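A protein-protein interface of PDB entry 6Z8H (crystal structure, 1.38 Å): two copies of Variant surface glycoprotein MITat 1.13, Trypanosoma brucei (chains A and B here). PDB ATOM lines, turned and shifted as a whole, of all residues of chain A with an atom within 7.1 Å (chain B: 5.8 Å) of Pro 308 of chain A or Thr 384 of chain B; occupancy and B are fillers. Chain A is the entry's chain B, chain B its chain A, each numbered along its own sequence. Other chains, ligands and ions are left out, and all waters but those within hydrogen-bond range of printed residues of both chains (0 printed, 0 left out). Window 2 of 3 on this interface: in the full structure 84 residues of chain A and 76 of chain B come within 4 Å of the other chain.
The backbone carbonyl oxygen (O) of Leu 380 of chain B sits at hydrogen-bond distance from the side-chain hydroxyl (OG1) of Thr 384 of chain B (3.0 Å). The guanidinium group of Arg 82 of chain A is in hydrogen-bond range of the backbone carbonyl oxygen of Ala 303 of chain A (2.8 Å). The side-chain amino group (NZ) of Lys 302 of chain A sits at hydrogen-bond distance from the backbone carbonyl oxygen (O) of Pro 308 of chain A (2.7 Å). The side-chain amino group (NZ) of Lys 302 of chain A is in hydrogen-bond range of the backbone carbonyl oxygen (O) of Ala 310 of chain A (2.9 Å). The side-chain amino group (NZ) of Lys 302 of chain A lies within salt-bridge range of the side-chain carboxylate (OE2) of Glu 311 of chain A, at 3.0 Å.
Ile 383 of chain B touches Arg 82 of chain A (CG2 to NH2, 3.1 Å). Leu 380 of chain B touches Lys 302 of chain A (CD2 to CB, 3.8 Å). CD2 of Leu 380 of chain B touches CB of Pro 308 of chain A (3.98 Å). Pro 308 of chain A touches Thr 384 of chain B (CG to OG1, 3.8 Å).
Printed residues of chain B within 4 Å of Arg 82 of chain A: Ile 383. Of the printed residues of chain B, Lys 302 of chain A touches Leu 380. Of the printed residues of chain A, Leu 380 of chain B touches Lys 302 and Pro 308. Glu 382 of chain B touches none of the printed residues of chain A. Printed residues of chain A within 4 Å of Ile 383 of chain B: Arg 82. The nearest printed residue of chain B that does not touch Pro 308 of chain A is Gln 381 of chain B (6.5 Å).
Printed residues of chain A that touch a printed residue of chain B: Arg 82, Lys 302 and Pro 308. Hydrophobic or aromatic side chains of chain A that line the printed part of chain B: Pro 308. Of the 6 printed residues of chain B, 3 touch a printed residue of chain A. Along chain B the printed residues that touch a printed residue of chain A span positions 380 to 384. Among the printed residues, 4 pairs touch across the chains. Among the printed residues, no Asp or Glu carboxylate lies within 4 Å of a Lys or Arg side-chain nitrogen of the other chain.
No position is printed for both chains.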
ATOM      1  N   ARG A  82       4.274   7.939  17.697  1.00  0.00           N
ATOM      2  CA  ARG A  82       4.755   8.825  16.650  1.00  0.00           C
ATOM      3  C   ARG A  82       4.831  10.270  17.131  1.00  0.00           C
ATOM      4  O   ARG A  82       5.689  11.027  16.675  1.00  0.00           O
ATOM      5  CB  ARG A  82       3.862   8.714  15.423  1.00  0.00           C
ATOM      6  CG  ARG A  82       4.061   7.424  14.701  1.00  0.00           C
ATOM      7  CD  ARG A  82       3.174   7.384  13.484  1.00  0.00           C
ATOM      8  NE  ARG A  82       3.304   6.160  12.702  1.00  0.00           N
ATOM      9  CZ  ARG A  82       4.261   5.935  11.803  1.00  0.00           C
ATOM     10  NH1 ARG A  82       5.179   6.868  11.577  1.00  0.00           N
ATOM     11  NH2 ARG A  82       4.281   4.785  11.123  1.00  0.00           N
ATOM     12  N   ILE A 301       9.423  14.889  10.372  1.00  0.00           N
ATOM     13  CA  ILE A 301       9.318  14.361   9.016  1.00  0.00           C
ATOM     14  C   ILE A 301       9.332  12.842   9.049  1.00  0.00           C
ATOM     15  O   ILE A 301       8.501  12.178   8.423  1.00  0.00           O
ATOM     16  CB  ILE A 301      10.466  14.901   8.148  1.00  0.00           C
ATOM     17  CG1 ILE A 301      10.376  16.422   8.006  1.00  0.00           C
ATOM     18  CG2 ILE A 301      10.467  14.208   6.785  1.00  0.00           C
ATOM     19  CD1 ILE A 301      11.512  17.038   7.235  1.00  0.00           C
ATOM     20  N   LYS A 302      10.282  12.265   9.781  1.00  0.00           N
ATOM     21  CA  LYS A 302      10.430  10.812   9.771  1.00  0.00           C
ATOM     22  C   LYS A 302       9.239  10.119  10.422  1.00  0.00           C
ATOM     23  O   LYS A 302       8.763   9.095   9.917  1.00  0.00           O
ATOM     24  CB  LYS A 302      11.723  10.400  10.481  1.00  0.00           C
ATOM     25  CG  LYS A 302      12.994  10.805   9.755  1.00  0.00           C
ATOM     26  CD  LYS A 302      14.247  10.706  10.643  1.00  0.00           C
ATOM     27  CE  LYS A 302      14.772   9.306  10.726  1.00  0.00           C
ATOM     28  NZ  LYS A 302      15.328   8.785   9.424  1.00  0.00           N
ATOM     29  N   ALA A 303       8.764  10.634  11.558  1.00  0.00           N
ATOM     30  CA  ALA A 303       7.749   9.945  12.341  1.00  0.00           C
ATOM     31  C   ALA A 303       6.324  10.391  12.039  1.00  0.00           C
ATOM     32  O   ALA A 303       5.399   9.587  12.190  1.00  0.00           O
ATOM     33  CB  ALA A 303       7.996  10.193  13.829  1.00  0.00           C
ATOM     34  N   LEU A 305       5.321  12.468   9.107  1.00  0.00           N
ATOM     35  CA  LEU A 305       5.025  12.683   7.693  1.00  0.00           C
ATOM     36  C   LEU A 305       5.232  11.428   6.844  1.00  0.00           C
ATOM     37  O   LEU A 305       5.248  11.508   5.615  1.00  0.00           O
ATOM     38  CB  LEU A 305       5.841  13.856   7.140  1.00  0.00           C
ATOM     39  CG  LEU A 305       5.387  15.223   7.655  1.00  0.00           C
ATOM     40  CD1 LEU A 305       6.130  16.386   6.999  1.00  0.00           C
ATOM     41  CD2 LEU A 305       3.886  15.413   7.469  1.00  0.00           C
ATOM     42  N   ASN A 306       5.397  10.272   7.473  1.00  0.00           N
ATOM     43  CA  ASN A 306       5.478   8.995   6.761  1.00  0.00           C
ATOM     44  C   ASN A 306       6.662   8.953   5.793  1.00  0.00           C
ATOM     45  O   ASN A 306       6.578   8.365   4.714  1.00  0.00           O
ATOM     46  CB  ASN A 306       4.164   8.681   6.039  1.00  0.00           C
ATOM     47  CG  ASN A 306       3.974   7.189   5.766  1.00  0.00           C
ATOM     48  OD1 ASN A 306       4.243   6.341   6.621  1.00  0.00           O
ATOM     49  ND2 ASN A 306       3.505   6.866   4.567  1.00  0.00           N
ATOM     50  N   LYS A 307       7.788   9.544   6.201  1.00  0.00           N
ATOM     51  CA  LYS A 307       9.031   9.524   5.425  1.00  0.00           C
ATOM     52  C   LYS A 307      10.166   9.037   6.330  1.00  0.00           C
ATOM     53  O   LYS A 307      11.065   9.807   6.707  1.00  0.00           O
ATOM     54  CB  LYS A 307       9.344  10.910   4.854  1.00  0.00           C
ATOM     55  CG  LYS A 307       8.266  11.529   3.967  1.00  0.00           C
ATOM     56  CD  LYS A 307       8.715  12.903   3.482  1.00  0.00           C
ATOM     57  CE  LYS A 307       7.606  13.661   2.779  1.00  0.00           C
ATOM     58  NZ  LYS A 307       7.174  12.963   1.565  1.00  0.00           N
ATOM     59  N   PRO A 308      10.154   7.753   6.702  1.00  0.00           N
ATOM     60  CA  PRO A 308      11.096   7.286   7.734  1.00  0.00           C
ATOM     61  C   PRO A 308      12.551   7.300   7.306  1.00  0.00           C
ATOM     62  O   PRO A 308      13.429   7.339   8.181  1.00  0.00           O
ATOM     63  CB  PRO A 308      10.628   5.858   8.056  1.00  0.00           C
ATOM     64  CG  PRO A 308       9.309   5.676   7.356  1.00  0.00           C
ATOM     65  CD  PRO A 308       9.263   6.686   6.229  1.00  0.00           C
ATOM     66  N   THR A 309      12.842   7.294   6.006  1.00  0.00           N
ATOM     67  CA  THR A 309      14.214   7.297   5.523  1.00  0.00           C
ATOM     68  C   THR A 309      14.772   8.697   5.345  1.00  0.00           C
ATOM     69  O   THR A 309      15.951   8.841   4.999  1.00  0.00           O
ATOM     70  CB  THR A 309      14.329   6.513   4.210  1.00  0.00           C
ATOM     71  OG1 THR A 309      13.518   7.120   3.196  1.00  0.00           O
ATOM     72  CG2 THR A 309      13.877   5.086   4.417  1.00  0.00           C
ATOM     73  N   ALA A 310      13.971   9.727   5.610  1.00  0.00           N
ATOM     74  CA  ALA A 310      14.444  11.092   5.457  1.00  0.00           C
ATOM     75  C   ALA A 310      15.612  11.363   6.395  1.00  0.00           C
ATOM     76  O   ALA A 310      15.618  10.938   7.556  1.00  0.00           O
ATOM     77  CB  ALA A 310      13.305  12.065   5.759  1.00  0.00           C
ATOM     78  N   GLU A 311      16.595  12.110   5.889  1.00  0.00           N
ATOM     79  CA  GLU A 311      17.700  12.573   6.709  1.00  0.00           C
ATOM     80  C   GLU A 311      17.968  14.065   6.582  1.00  0.00           C
ATOM     81  O   GLU A 311      18.932  14.557   7.186  1.00  0.00           O
ATOM     82  CB  GLU A 311      18.980  11.813   6.369  1.00  0.00           C
ATOM     83  CG  GLU A 311      18.899  10.315   6.653  1.00  0.00           C
ATOM     84  CD  GLU A 311      18.790   9.966   8.137  1.00  0.00           C
ATOM     85  OE1 GLU A 311      19.372  10.686   8.983  1.00  0.00           O
ATOM     86  OE2 GLU A 311      18.119   8.957   8.467  1.00  0.00           O
ATOM     87  N   LEU B 379      12.875   2.616  17.452  1.00  0.00           N
ATOM     88  CA  LEU B 379      11.443   2.439  17.657  1.00  0.00           C
ATOM     89  C   LEU B 379      10.674   2.729  16.373  1.00  0.00           C
ATOM     90  O   LEU B 379       9.674   2.060  16.067  1.00  0.00           O
ATOM     91  CB  LEU B 379      10.968   3.313  18.814  1.00  0.00           C
ATOM     92  CG  LEU B 379      11.523   2.988  20.205  1.00  0.00           C
ATOM     93  CD1 LEU B 379      11.159   4.065  21.172  1.00  0.00           C
ATOM     94  CD2 LEU B 379      10.998   1.654  20.679  1.00  0.00           C
ATOM     95  N   LEU B 380      11.125   3.717  15.595  1.00  0.00           N
ATOM     96  CA  LEU B 380      10.457   4.006  14.333  1.00  0.00           C
ATOM     97  C   LEU B 380      10.583   2.815  13.398  1.00  0.00           C
ATOM     98  O   LEU B 380       9.630   2.443  12.704  1.00  0.00           O
ATOM     99  CB  LEU B 380      11.053   5.266  13.703  1.00  0.00           C
ATOM    100  CG  LEU B 380      10.459   5.724  12.366  1.00  0.00           C
ATOM    101  CD1 LEU B 380       8.973   5.963  12.530  1.00  0.00           C
ATOM    102  CD2 LEU B 380      11.174   6.938  11.848  1.00  0.00           C
ATOM    103  N   GLN B 381      11.762   2.201  13.370  1.00  0.00           N
ATOM    104  CA  GLN B 381      11.953   1.002  12.567  1.00  0.00           C
ATOM    105  C   GLN B 381      10.913  -0.056  12.907  1.00  0.00           C
ATOM    106  O   GLN B 381      10.353  -0.707  12.017  1.00  0.00           O
ATOM    107  CB  GLN B 381      13.352   0.450  12.809  1.00  0.00           C
ATOM    108  CG  GLN B 381      13.614  -0.866  12.093  1.00  0.00           C
ATOM    109  CD  GLN B 381      14.256  -0.654  10.733  1.00  0.00           C
ATOM    110  OE1 GLN B 381      13.659  -0.047   9.833  1.00  0.00           O
ATOM    111  NE2 GLN B 381      15.491  -1.138  10.583  1.00  0.00           N
ATOM    112  N   GLU B 382      10.677  -0.281  14.198  1.00  0.00           N
ATOM    113  CA  GLU B 382       9.730  -1.322  14.580  1.00  0.00           C
ATOM    114  C   GLU B 382       8.308  -0.936  14.192  1.00  0.00           C
ATOM    115  O   GLU B 382       7.507  -1.801  13.827  1.00  0.00           O
ATOM    116  CB  GLU B 382       9.852  -1.627  16.076  1.00  0.00           C
ATOM    117  CG  GLU B 382       9.499  -3.067  16.431  1.00  0.00           C
ATOM    118  CD  GLU B 382      10.394  -4.100  15.736  1.00  0.00           C
ATOM    119  OE1 GLU B 382      11.449  -3.699  15.188  1.00  0.00           O
ATOM    120  OE2 GLU B 382      10.043  -5.304  15.736  1.00  0.00           O
ATOM    121  N   ILE B 383       7.976   0.354  14.245  1.00  0.00           N
ATOM    122  CA  ILE B 383       6.680   0.815  13.745  1.00  0.00           C
ATOM    123  C   ILE B 383       6.582   0.588  12.241  1.00  0.00           C
ATOM    124  O   ILE B 383       5.578   0.076  11.730  1.00  0.00           O
ATOM    125  CB  ILE B 383       6.472   2.296  14.124  1.00  0.00           C
ATOM    126  CG1 ILE B 383       6.347   2.421  15.640  1.00  0.00           C
ATOM    127  CG2 ILE B 383       5.245   2.864  13.423  1.00  0.00           C
ATOM    128  CD1 ILE B 383       6.525   3.808  16.131  1.00  0.00           C
ATOM    129  N   THR B 384       7.639   0.938  11.514  1.00  0.00           N
ATOM    130  CA  THR B 384       7.698   0.747  10.072  1.00  0.00           C
ATOM    131  C   THR B 384       7.741  -0.745   9.742  1.00  0.00           C
ATOM    132  O   THR B 384       6.879  -1.259   9.036  1.00  0.00           O
ATOM    133  CB  THR B 384       8.931   1.436   9.457  1.00  0.00           C
ATOM    134  OG1 THR B 384       8.934   2.833   9.786  1.00  0.00           O
ATOM    135  CG2 THR B 384       8.929   1.275   7.947  1.00  0.00           C
